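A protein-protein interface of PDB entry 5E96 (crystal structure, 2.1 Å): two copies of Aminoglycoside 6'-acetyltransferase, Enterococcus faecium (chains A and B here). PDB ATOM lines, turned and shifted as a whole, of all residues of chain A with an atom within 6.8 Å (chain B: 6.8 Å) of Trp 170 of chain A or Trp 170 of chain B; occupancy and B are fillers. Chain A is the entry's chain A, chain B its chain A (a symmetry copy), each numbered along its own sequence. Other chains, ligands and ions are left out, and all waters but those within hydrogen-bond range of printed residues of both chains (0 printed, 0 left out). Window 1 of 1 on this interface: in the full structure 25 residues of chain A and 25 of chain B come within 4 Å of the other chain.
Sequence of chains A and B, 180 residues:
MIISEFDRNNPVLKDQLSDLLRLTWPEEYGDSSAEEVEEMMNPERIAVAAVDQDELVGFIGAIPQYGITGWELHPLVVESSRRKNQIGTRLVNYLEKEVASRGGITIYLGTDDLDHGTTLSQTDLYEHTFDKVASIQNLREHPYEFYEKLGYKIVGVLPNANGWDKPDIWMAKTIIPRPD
Of the 16 printed residues of chain B, 9 touch a printed residue of chain A. Hydrophobic or aromatic side chains of chain B within 4 Å of the printed part of chain A: Tyr 66, Tyr 108, Val 155, Leu 158, Trp 170 and Ala 172. Hydrophobic or aromatic side chains of chain A that line the printed part of chain B: Tyr 66, Tyr 108, Val 155, Leu 158, Trp 170 and Ala 172. Among the printed residues, 20 pairs touch across the chains. Among the printed residues, no Asp or Glu carboxylate lies within 4 Å of a Lys or Arg side-chain nitrogen of the other chain.
Printed residues of chain B within 4 Å of Gly 156 of chain A: Val 155 (3.2 Å) and Gly 156 (3.6 Å). Of the printed residues of chain B, Asp 168 of chain A touches Tyr 66. Of the printed residues of chain A, Val 155 of chain B touches Gly 156 (3.2 Å), Val 157 (2.9 Å) and Trp 170 (3.5 Å). Of the printed residues of chain A, Leu 158 of chain B touches Tyr 66 (3.8 Å), Tyr 108 (3.7 Å) and Ala 172 (3.5 Å). Of chain A, only Tyr 66, Tyr 108, Val 155 and Trp 170 come within 4 Å of Trp 170 of chain B. The nearest residue of chain B that does not touch Trp 170 of chain A is Gly 156 of chain B (4.7 Å). The nearest printed residue of chain A that does not touch Tyr 66 of chain B is Gly 110 of chain A (4.9 Å).
NE1 of Trp 170 of chain B is in hydrogen-bond range of OH of Tyr 66 of chain A (3.2 Å). The backbone carbonyl oxygen of Val 155 of chain A sits at hydrogen-bond distance from the backbone NH of Val 157 of chain B, 2.9 Å away. N of Val 157 of chain A lies within hydrogen-bond range of O of Val 155 of chain B (2.9 Å). The indole nitrogen (NE1) of Trp 170 of chain A sits at hydrogen-bond distance from the side-chain hydroxyl (OH) of Tyr 66 of chain B, at 3.2 Å.
Tyr 66 of chain A touches Trp 170 of chain B, and with the chains exchanged Trp 170 of chain A touches Tyr 66 of chain B. Tyr 108 of chain A touches Trp 170 of chain B, and with the chains exchanged Trp 170 of chain A touches Tyr 108 of chain B. Val 155 of chain A touches Trp 170 of chain B, and with the chains exchanged Trp 170 of chain A touches Val 155 of chain B. Gly 156 of chain B touches its own counterpart, Gly 156 of chain A. 16 positions are printed for both chains.
N of Thr 111 of chain A sits at hydrogen-bond distance from OD2 of Asp 168 of chain A (3.2 Å). The backbone NH (N) of Val 155 of chain A sits at hydrogen-bond distance from the backbone carbonyl oxygen (O) of Trp 170 of chain A (2.8 Å). The backbone NH (N) of Leu 158 of chain A lies within hydrogen-bond range of the backbone carbonyl oxygen (O) of Asp 168 of chain A (3.0 Å). N of Thr 111 of chain B is in hydrogen-bond range of OD2 of Asp 168 of chain B (3.2 Å). The backbone NH of Val 155 of chain B is in hydrogen-bond range of the backbone carbonyl oxygen of Trp 170 of chain B. The backbone NH (N) of Leu 158 of chain B lies within hydrogen-bond range of the backbone carbonyl oxygen (O) of Asp 168 of chain B, 3.0 Å away.
OD2 of Asp 168 of chain B touches CE1 of Tyr 66 of chain A, 3.1 Å away. CD2 of Tyr 108 of chain A touches CZ2 of Trp 170 of chain B (3.9 Å). Val 155 of chain A touches Gly 156 of chain B (O to CA, 3.2 Å). Val 155 of chain A touches Trp 170 of chain B (CG2 to CZ3, 3.5 Å). Leu 158 of chain A touches Tyr 66 of chain B (CD2 to CE2, 3.8 Å). Leu 158 of chain A touches Tyr 108 of chain B. CD1 of Leu 158 of chain A touches CB of Ala 172 of chain B, 3.5 Å away. Asp 168 of chain A touches Tyr 66 of chain B (OD2 to CE1, 3.1 Å). Trp 170 of chain A touches Tyr 108 of chain B. Trp 170 of chain A touches Val 155 of chain B.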
ATOM      1  N   TYR A  66     -13.316   0.076  -2.291  1.00  0.00           N
ATOM      2  CA  TYR A  66     -12.220  -0.864  -2.492  1.00  0.00           C
ATOM      3  C   TYR A  66     -11.852  -1.475  -1.146  1.00  0.00           C
ATOM      4  O   TYR A  66     -11.070  -0.900  -0.385  1.00  0.00           O
ATOM      5  CB  TYR A  66     -11.021  -0.130  -3.104  1.00  0.00           C
ATOM      6  CG  TYR A  66     -11.393   0.637  -4.352  1.00  0.00           C
ATOM      7  CD1 TYR A  66     -11.788  -0.032  -5.515  1.00  0.00           C
ATOM      8  CD2 TYR A  66     -11.417   2.030  -4.357  1.00  0.00           C
ATOM      9  CE1 TYR A  66     -12.203   0.669  -6.650  1.00  0.00           C
ATOM     10  CE2 TYR A  66     -11.833   2.741  -5.487  1.00  0.00           C
ATOM     11  CZ  TYR A  66     -12.224   2.053  -6.628  1.00  0.00           C
ATOM     12  OH  TYR A  66     -12.636   2.752  -7.743  1.00  0.00           O
ATOM     13  N   TYR A 108     -11.428   9.238  -1.861  1.00  0.00           N
ATOM     14  CA  TYR A 108     -11.513   9.932  -3.137  1.00  0.00           C
ATOM     15  C   TYR A 108     -12.920  10.451  -3.320  1.00  0.00           C
ATOM     16  O   TYR A 108     -13.839  10.069  -2.596  1.00  0.00           O
ATOM     17  CB  TYR A 108     -11.153   9.011  -4.313  1.00  0.00           C
ATOM     18  CG  TYR A 108     -12.190   7.962  -4.638  1.00  0.00           C
ATOM     19  CD1 TYR A 108     -12.314   6.819  -3.860  1.00  0.00           C
ATOM     20  CD2 TYR A 108     -13.063   8.125  -5.715  1.00  0.00           C
ATOM     21  CE1 TYR A 108     -13.280   5.854  -4.142  1.00  0.00           C
ATOM     22  CE2 TYR A 108     -14.041   7.165  -6.006  1.00  0.00           C
ATOM     23  CZ  TYR A 108     -14.137   6.036  -5.211  1.00  0.00           C
ATOM     24  OH  TYR A 108     -15.098   5.086  -5.469  1.00  0.00           O
ATOM     25  N   LEU A 109     -13.082  11.321  -4.302  1.00  0.00           N
ATOM     26  CA  LEU A 109     -14.376  11.903  -4.588  1.00  0.00           C
ATOM     27  C   LEU A 109     -14.439  12.364  -6.042  1.00  0.00           C
ATOM     28  O   LEU A 109     -13.409  12.535  -6.703  1.00  0.00           O
ATOM     29  CB  LEU A 109     -14.605  13.091  -3.649  1.00  0.00           C
ATOM     30  CG  LEU A 109     -13.557  14.203  -3.794  1.00  0.00           C
ATOM     31  CD1 LEU A 109     -14.060  15.221  -4.825  1.00  0.00           C
ATOM     32  CD2 LEU A 109     -13.303  14.877  -2.440  1.00  0.00           C
ATOM     33  N   GLY A 110     -15.656  12.560  -6.532  1.00  0.00           N
ATOM     34  CA  GLY A 110     -15.840  13.047  -7.880  1.00  0.00           C
ATOM     35  C   GLY A 110     -16.615  14.344  -7.790  1.00  0.00           C
ATOM     36  O   GLY A 110     -17.549  14.456  -6.996  1.00  0.00           O
ATOM     37  N   THR A 111     -16.229  15.341  -8.576  1.00  0.00           N
ATOM     38  CA  THR A 111     -16.942  16.608  -8.553  1.00  0.00           C
ATOM     39  C   THR A 111     -16.981  17.233  -9.931  1.00  0.00           C
ATOM     40  O   THR A 111     -16.039  17.092 -10.710  1.00  0.00           O
ATOM     41  CB  THR A 111     -16.286  17.625  -7.579  1.00  0.00           C
ATOM     42  OG1 THR A 111     -17.037  18.848  -7.602  1.00  0.00           O
ATOM     43  CG2 THR A 111     -14.834  17.919  -7.988  1.00  0.00           C
ATOM     44  N   LYS A 153      -5.943  15.929  -3.873  1.00  0.00           N
ATOM     45  CA  LYS A 153      -5.276  16.158  -5.155  1.00  0.00           C
ATOM     46  C   LYS A 153      -5.962  15.448  -6.324  1.00  0.00           C
ATOM     47  O   LYS A 153      -6.527  14.361  -6.177  1.00  0.00           O
ATOM     48  CB  LYS A 153      -3.816  15.708  -5.053  1.00  0.00           C
ATOM     49  CG  LYS A 153      -3.059  16.384  -3.911  1.00  0.00           C
ATOM     50  CD  LYS A 153      -1.641  15.865  -3.789  1.00  0.00           C
ATOM     51  CE  LYS A 153      -0.910  16.519  -2.618  1.00  0.00           C
ATOM     52  N   ILE A 154      -5.913  16.071  -7.488  1.00  0.00           N
ATOM     53  CA  ILE A 154      -6.544  15.484  -8.654  1.00  0.00           C
ATOM     54  C   ILE A 154      -5.877  14.162  -9.004  1.00  0.00           C
ATOM     55  O   ILE A 154      -4.665  14.114  -9.181  1.00  0.00           O
ATOM     56  CB  ILE A 154      -6.437  16.408  -9.858  1.00  0.00           C
ATOM     57  CG1 ILE A 154      -7.157  17.719  -9.549  1.00  0.00           C
ATOM     58  CG2 ILE A 154      -7.014  15.711 -11.094  1.00  0.00           C
ATOM     59  CD1 ILE A 154      -7.051  18.758 -10.651  1.00  0.00           C
ATOM     60  N   VAL A 155      -6.666  13.093  -9.084  1.00  0.00           N
ATOM     61  CA  VAL A 155      -6.124  11.784  -9.437  1.00  0.00           C
ATOM     62  C   VAL A 155      -6.731  11.262 -10.738  1.00  0.00           C
ATOM     63  O   VAL A 155      -6.454  10.143 -11.154  1.00  0.00           O
ATOM     64  CB  VAL A 155      -6.367  10.758  -8.319  1.00  0.00           C
ATOM     65  CG1 VAL A 155      -5.529  11.125  -7.095  1.00  0.00           C
ATOM     66  CG2 VAL A 155      -7.855  10.720  -7.957  1.00  0.00           C
ATOM     67  N   GLY A 156      -7.558  12.076 -11.383  1.00  0.00           N
ATOM     68  CA  GLY A 156      -8.163  11.645 -12.632  1.00  0.00           C
ATOM     69  C   GLY A 156      -9.199  12.619 -13.150  1.00  0.00           C
ATOM     70  O   GLY A 156      -9.710  13.451 -12.399  1.00  0.00           O
ATOM     71  N   VAL A 157      -9.503  12.521 -14.439  1.00  0.00           N
ATOM     72  CA  VAL A 157     -10.486  13.388 -15.067  1.00  0.00           C
ATOM     73  C   VAL A 157     -11.295  12.579 -16.082  1.00  0.00           C
ATOM     74  O   VAL A 157     -10.740  11.778 -16.831  1.00  0.00           O
ATOM     75  CB  VAL A 157      -9.805  14.581 -15.805  1.00  0.00           C
ATOM     76  CG1 VAL A 157     -10.876  15.481 -16.430  1.00  0.00           C
ATOM     77  CG2 VAL A 157      -8.940  15.388 -14.832  1.00  0.00           C
ATOM     78  N   LEU A 158     -12.607  12.776 -16.100  1.00  0.00           N
ATOM     79  CA  LEU A 158     -13.460  12.067 -17.048  1.00  0.00           C
ATOM     80  C   LEU A 158     -14.105  13.064 -17.995  1.00  0.00           C
ATOM     81  O   LEU A 158     -15.049  13.766 -17.624  1.00  0.00           O
ATOM     82  CB  LEU A 158     -14.550  11.274 -16.312  1.00  0.00           C
ATOM     83  CG  LEU A 158     -15.589  10.585 -17.205  1.00  0.00           C
ATOM     84  CD1 LEU A 158     -14.890   9.578 -18.122  1.00  0.00           C
ATOM     85  CD2 LEU A 158     -16.642   9.884 -16.348  1.00  0.00           C
ATOM     86  N   ASP A 168     -15.800  15.579 -15.132  1.00  0.00           N
ATOM     87  CA  ASP A 168     -15.946  15.386 -13.710  1.00  0.00           C
ATOM     88  C   ASP A 168     -14.506  15.174 -13.271  1.00  0.00           C
ATOM     89  O   ASP A 168     -13.741  14.472 -13.944  1.00  0.00           O
ATOM     90  CB  ASP A 168     -16.795  14.160 -13.388  1.00  0.00           C
ATOM     91  CG  ASP A 168     -17.687  14.388 -12.187  1.00  0.00           C
ATOM     92  OD1 ASP A 168     -18.617  15.207 -12.298  1.00  0.00           O
ATOM     93  OD2 ASP A 168     -17.454  13.768 -11.132  1.00  0.00           O
ATOM     94  N   ILE A 169     -14.122  15.805 -12.171  1.00  0.00           N
ATOM     95  CA  ILE A 169     -12.761  15.674 -11.681  1.00  0.00           C
ATOM     96  C   ILE A 169     -12.739  14.784 -10.449  1.00  0.00           C
ATOM     97  O   ILE A 169     -13.573  14.927  -9.557  1.00  0.00           O
ATOM     98  CB  ILE A 169     -12.148  17.067 -11.338  1.00  0.00           C
ATOM     99  CG1 ILE A 169     -11.843  17.845 -12.624  1.00  0.00           C
ATOM    100  CG2 ILE A 169     -10.870  16.902 -10.538  1.00  0.00           C
ATOM    101  CD1 ILE A 169     -13.071  18.297 -13.393  1.00  0.00           C
ATOM    102  N   TRP A 170     -11.797  13.849 -10.418  1.00  0.00           N
ATOM    103  CA  TRP A 170     -11.658  12.956  -9.285  1.00  0.00           C
ATOM    104  C   TRP A 170     -10.484  13.441  -8.450  1.00  0.00           C
ATOM    105  O   TRP A 170      -9.399  13.714  -8.982  1.00  0.00           O
ATOM    106  CB  TRP A 170     -11.398  11.517  -9.742  1.00  0.00           C
ATOM    107  CG  TRP A 170     -12.558  10.865 -10.440  1.00  0.00           C
ATOM    108  CD1 TRP A 170     -13.845  10.794  -9.995  1.00  0.00           C
ATOM    109  CD2 TRP A 170     -12.521  10.130 -11.672  1.00  0.00           C
ATOM    110  NE1 TRP A 170     -14.612  10.056 -10.866  1.00  0.00           N
ATOM    111  CE2 TRP A 170     -13.824   9.634 -11.904  1.00  0.00           C
ATOM    112  CE3 TRP A 170     -11.514   9.838 -12.598  1.00  0.00           C
ATOM    113  CZ2 TRP A 170     -14.146   8.861 -13.026  1.00  0.00           C
ATOM    114  CZ3 TRP A 170     -11.835   9.065 -13.716  1.00  0.00           C
ATOM    115  CH2 TRP A 170     -13.144   8.586 -13.914  1.00  0.00           C
ATOM    116  N   MET A 171     -10.710  13.550  -7.145  1.00  0.00           N
ATOM    117  CA  MET A 171      -9.685  14.002  -6.216  1.00  0.00           C
ATOM    118  C   MET A 171      -9.555  12.960  -5.110  1.00  0.00           C
ATOM    119  O   MET A 171     -10.513  12.242  -4.804  1.00  0.00           O
ATOM    120  CB  MET A 171     -10.077  15.369  -5.641  1.00  0.00           C
ATOM    121  CG  MET A 171     -10.295  16.434  -6.716  1.00  0.00           C
ATOM    122  SD  MET A 171     -10.820  18.071  -6.100  1.00  0.00           S
ATOM    123  CE  MET A 171      -9.267  18.666  -5.385  1.00  0.00           C
ATOM    124  N   ALA A 172      -8.371  12.868  -4.515  1.00  0.00           N
ATOM    125  CA  ALA A 172      -8.138  11.886  -3.469  1.00  0.00           C
ATOM    126  C   ALA A 172      -7.071  12.332  -2.480  1.00  0.00           C
ATOM    127  O   ALA A 172      -6.295  13.253  -2.746  1.00  0.00           O
ATOM    128  CB  ALA A 172      -7.742  10.536  -4.099  1.00  0.00           C
ATOM    129  N   TYR B  66     -23.391  10.027 -13.785  1.00  0.00           N
ATOM    130  CA  TYR B  66     -23.434  11.453 -14.087  1.00  0.00           C
ATOM    131  C   TYR B  66     -24.575  11.707 -15.065  1.00  0.00           C
ATOM    132  O   TYR B  66     -24.408  11.569 -16.279  1.00  0.00           O
ATOM    133  CB  TYR B  66     -22.093  11.887 -14.690  1.00  0.00           C
ATOM    134  CG  TYR B  66     -20.919  11.491 -13.825  1.00  0.00           C
ATOM    135  CD1 TYR B  66     -20.728  12.065 -12.564  1.00  0.00           C
ATOM    136  CD2 TYR B  66     -20.034  10.494 -14.231  1.00  0.00           C
ATOM    137  CE1 TYR B  66     -19.688  11.652 -11.728  1.00  0.00           C
ATOM    138  CE2 TYR B  66     -18.992  10.071 -13.401  1.00  0.00           C
ATOM    139  CZ  TYR B  66     -18.826  10.655 -12.152  1.00  0.00           C
ATOM    140  OH  TYR B  66     -17.799  10.240 -11.332  1.00  0.00           O
ATOM    141  N   TYR B 108     -17.086   4.638 -18.132  1.00  0.00           N
ATOM    142  CA  TYR B 108     -15.828   4.484 -17.417  1.00  0.00           C
ATOM    143  C   TYR B 108     -15.922   3.274 -16.516  1.00  0.00           C
ATOM    144  O   TYR B 108     -17.003   2.735 -16.284  1.00  0.00           O
ATOM    145  CB  TYR B 108     -15.496   5.724 -16.570  1.00  0.00           C
ATOM    146  CG  TYR B 108     -16.355   5.900 -15.339  1.00  0.00           C
ATOM    147  CD1 TYR B 108     -17.650   6.389 -15.439  1.00  0.00           C
ATOM    148  CD2 TYR B 108     -15.875   5.556 -14.075  1.00  0.00           C
ATOM    149  CE1 TYR B 108     -18.455   6.539 -14.312  1.00  0.00           C
ATOM    150  CE2 TYR B 108     -16.676   5.698 -12.933  1.00  0.00           C
ATOM    151  CZ  TYR B 108     -17.962   6.189 -13.068  1.00  0.00           C
ATOM    152  OH  TYR B 108     -18.771   6.324 -11.963  1.00  0.00           O
ATOM    153  N   LEU B 109     -14.776   2.857 -16.004  1.00  0.00           N
ATOM    154  CA  LEU B 109     -14.717   1.706 -15.128  1.00  0.00           C
ATOM    155  C   LEU B 109     -13.482   1.786 -14.234  1.00  0.00           C
ATOM    156  O   LEU B 109     -12.534   2.526 -14.519  1.00  0.00           O
ATOM    157  CB  LEU B 109     -14.669   0.436 -15.980  1.00  0.00           C
ATOM    158  CG  LEU B 109     -13.455   0.365 -16.916  1.00  0.00           C
ATOM    159  CD1 LEU B 109     -12.315  -0.361 -16.190  1.00  0.00           C
ATOM    160  CD2 LEU B 109     -13.824  -0.362 -18.215  1.00  0.00           C
ATOM    161  N   GLY B 110     -13.504   1.018 -13.151  1.00  0.00           N
ATOM    162  CA  GLY B 110     -12.370   0.969 -12.258  1.00  0.00           C
ATOM    163  C   GLY B 110     -11.900  -0.469 -12.201  1.00  0.00           C
ATOM    164  O   GLY B 110     -12.719  -1.387 -12.158  1.00  0.00           O
ATOM    165  N   THR B 111     -10.592  -0.685 -12.226  1.00  0.00           N
ATOM    166  CA  THR B 111     -10.074  -2.041 -12.155  1.00  0.00           C
ATOM    167  C   THR B 111      -8.775  -2.087 -11.380  1.00  0.00           C
ATOM    168  O   THR B 111      -7.983  -1.147 -11.430  1.00  0.00           O
ATOM    169  CB  THR B 111      -9.815  -2.637 -13.566  1.00  0.00           C
ATOM    170  OG1 THR B 111      -9.310  -3.974 -13.426  1.00  0.00           O
ATOM    171  CG2 THR B 111      -8.792  -1.792 -14.340  1.00  0.00           C
ATOM    172  N   LYS B 153      -9.341   4.040 -22.442  1.00  0.00           N
ATOM    173  CA  LYS B 153      -8.085   4.697 -22.079  1.00  0.00           C
ATOM    174  C   LYS B 153      -8.030   5.117 -20.607  1.00  0.00           C
ATOM    175  O   LYS B 153      -9.042   5.476 -20.001  1.00  0.00           O
ATOM    176  CB  LYS B 153      -7.874   5.917 -22.980  1.00  0.00           C
ATOM    177  CG  LYS B 153      -7.905   5.575 -24.468  1.00  0.00           C
ATOM    178  CD  LYS B 153      -7.767   6.810 -25.334  1.00  0.00           C
ATOM    179  CE  LYS B 153      -7.842   6.458 -26.819  1.00  0.00           C
ATOM    180  N   ILE B 154      -6.840   5.064 -20.036  1.00  0.00           N
ATOM    181  CA  ILE B 154      -6.687   5.432 -18.641  1.00  0.00           C
ATOM    182  C   ILE B 154      -7.041   6.897 -18.441  1.00  0.00           C
ATOM    183  O   ILE B 154      -6.484   7.760 -19.110  1.00  0.00           O
ATOM    184  CB  ILE B 154      -5.256   5.216 -18.172  1.00  0.00           C
ATOM    185  CG1 ILE B 154      -4.902   3.735 -18.307  1.00  0.00           C
ATOM    186  CG2 ILE B 154      -5.106   5.715 -16.733  1.00  0.00           C
ATOM    187  CD1 ILE B 154      -3.466   3.407 -17.943  1.00  0.00           C
ATOM    188  N   VAL B 155      -7.978   7.171 -17.537  1.00  0.00           N
ATOM    189  CA  VAL B 155      -8.370   8.549 -17.254  1.00  0.00           C
ATOM    190  C   VAL B 155      -8.077   8.927 -15.804  1.00  0.00           C
ATOM    191  O   VAL B 155      -8.408  10.021 -15.362  1.00  0.00           O
ATOM    192  CB  VAL B 155      -9.862   8.776 -17.544  1.00  0.00           C
ATOM    193  CG1 VAL B 155     -10.115   8.678 -19.048  1.00  0.00           C
ATOM    194  CG2 VAL B 155     -10.705   7.740 -16.792  1.00  0.00           C
ATOM    195  N   GLY B 156      -7.450   8.021 -15.064  1.00  0.00           N
ATOM    196  CA  GLY B 156      -7.131   8.320 -13.678  1.00  0.00           C
ATOM    197  C   GLY B 156      -6.567   7.129 -12.934  1.00  0.00           C
ATOM    198  O   GLY B 156      -6.732   5.985 -13.363  1.00  0.00           O
ATOM    199  N   VAL B 157      -5.893   7.397 -11.822  1.00  0.00           N
ATOM    200  CA  VAL B 157      -5.303   6.349 -11.006  1.00  0.00           C
ATOM    201  C   VAL B 157      -5.461   6.712  -9.530  1.00  0.00           C
ATOM    202  O   VAL B 157      -5.261   7.862  -9.141  1.00  0.00           O
ATOM    203  CB  VAL B 157      -3.786   6.168 -11.319  1.00  0.00           C
ATOM    204  CG1 VAL B 157      -3.212   5.040 -10.456  1.00  0.00           C
ATOM    205  CG2 VAL B 157      -3.580   5.855 -12.804  1.00  0.00           C
ATOM    206  N   LEU B 158      -5.833   5.739  -8.707  1.00  0.00           N
ATOM    207  CA  LEU B 158      -5.989   5.984  -7.277  1.00  0.00           C
ATOM    208  C   LEU B 158      -4.973   5.157  -6.507  1.00  0.00           C
ATOM    209  O   LEU B 158      -5.137   3.946  -6.347  1.00  0.00           O
ATOM    210  CB  LEU B 158      -7.408   5.622  -6.814  1.00  0.00           C
ATOM    211  CG  LEU B 158      -7.659   5.717  -5.304  1.00  0.00           C
ATOM    212  CD1 LEU B 158      -7.423   7.154  -4.834  1.00  0.00           C
ATOM    213  CD2 LEU B 158      -9.085   5.276  -4.976  1.00  0.00           C
ATOM    214  N   ASP B 168      -5.923   1.425  -8.105  1.00  0.00           N
ATOM    215  CA  ASP B 168      -7.047   1.032  -8.921  1.00  0.00           C
ATOM    216  C   ASP B 168      -6.914   1.969 -10.111  1.00  0.00           C
ATOM    217  O   ASP B 168      -6.619   3.159  -9.945  1.00  0.00           O
ATOM    218  CB  ASP B 168      -8.374   1.257  -8.203  1.00  0.00           C
ATOM    219  CG  ASP B 168      -9.372   0.158  -8.501  1.00  0.00           C
ATOM    220  OD1 ASP B 168      -9.135  -0.980  -8.058  1.00  0.00           O
ATOM    221  OD2 ASP B 168     -10.378   0.422  -9.187  1.00  0.00           O
ATOM    222  N   ILE B 169      -7.091   1.434 -11.310  1.00  0.00           N
ATOM    223  CA  ILE B 169      -6.972   2.246 -12.508  1.00  0.00           C
ATOM    224  C   ILE B 169      -8.350   2.512 -13.092  1.00  0.00           C
ATOM    225  O   ILE B 169      -9.174   1.605 -13.192  1.00  0.00           O
ATOM    226  CB  ILE B 169      -6.070   1.550 -13.574  1.00  0.00           C
ATOM    227  CG1 ILE B 169      -4.601   1.590 -13.136  1.00  0.00           C
ATOM    228  CG2 ILE B 169      -6.210   2.239 -14.918  1.00  0.00           C
ATOM    229  CD1 ILE B 169      -4.279   0.721 -11.934  1.00  0.00           C
ATOM    230  N   TRP B 170      -8.603   3.764 -13.453  1.00  0.00           N
ATOM    231  CA  TRP B 170      -9.872   4.137 -14.046  1.00  0.00           C
ATOM    232  C   TRP B 170      -9.659   4.290 -15.542  1.00  0.00           C
ATOM    233  O   TRP B 170      -8.710   4.954 -15.983  1.00  0.00           O
ATOM    234  CB  TRP B 170     -10.387   5.458 -13.467  1.00  0.00           C
ATOM    235  CG  TRP B 170     -10.791   5.390 -12.019  1.00  0.00           C
ATOM    236  CD1 TRP B 170     -11.632   4.481 -11.449  1.00  0.00           C
ATOM    237  CD2 TRP B 170     -10.430   6.309 -10.978  1.00  0.00           C
ATOM    238  NE1 TRP B 170     -11.824   4.777 -10.120  1.00  0.00           N
ATOM    239  CE2 TRP B 170     -11.099   5.896  -9.805  1.00  0.00           C
ATOM    240  CE3 TRP B 170      -9.611   7.441 -10.925  1.00  0.00           C
ATOM    241  CZ2 TRP B 170     -10.975   6.578  -8.588  1.00  0.00           C
ATOM    242  CZ3 TRP B 170      -9.488   8.123  -9.713  1.00  0.00           C
ATOM    243  CH2 TRP B 170     -10.171   7.684  -8.563  1.00  0.00           C
ATOM    244  N   MET B 171     -10.543   3.671 -16.316  1.00  0.00           N
ATOM    245  CA  MET B 171     -10.473   3.722 -17.770  1.00  0.00           C
ATOM    246  C   MET B 171     -11.822   4.204 -18.293  1.00  0.00           C
ATOM    247  O   MET B 171     -12.856   4.004 -17.646  1.00  0.00           O
ATOM    248  CB  MET B 171     -10.133   2.332 -18.320  1.00  0.00           C
ATOM    249  CG  MET B 171      -8.822   1.769 -17.767  1.00  0.00           C
ATOM    250  SD  MET B 171      -8.388   0.092 -18.339  1.00  0.00           S
ATOM    251  CE  MET B 171      -7.879   0.446 -20.040  1.00  0.00           C
ATOM    252  N   ALA B 172     -11.816   4.844 -19.457  1.00  0.00           N
ATOM    253  CA  ALA B 172     -13.047   5.366 -20.026  1.00  0.00           C
ATOM    254  C   ALA B 172     -13.004   5.430 -21.545  1.00  0.00           C
ATOM    255  O   ALA B 172     -11.937   5.359 -22.160  1.00  0.00           O
ATOM    256  CB  ALA B 172     -13.339   6.763 -19.446  1.00  0.00           C
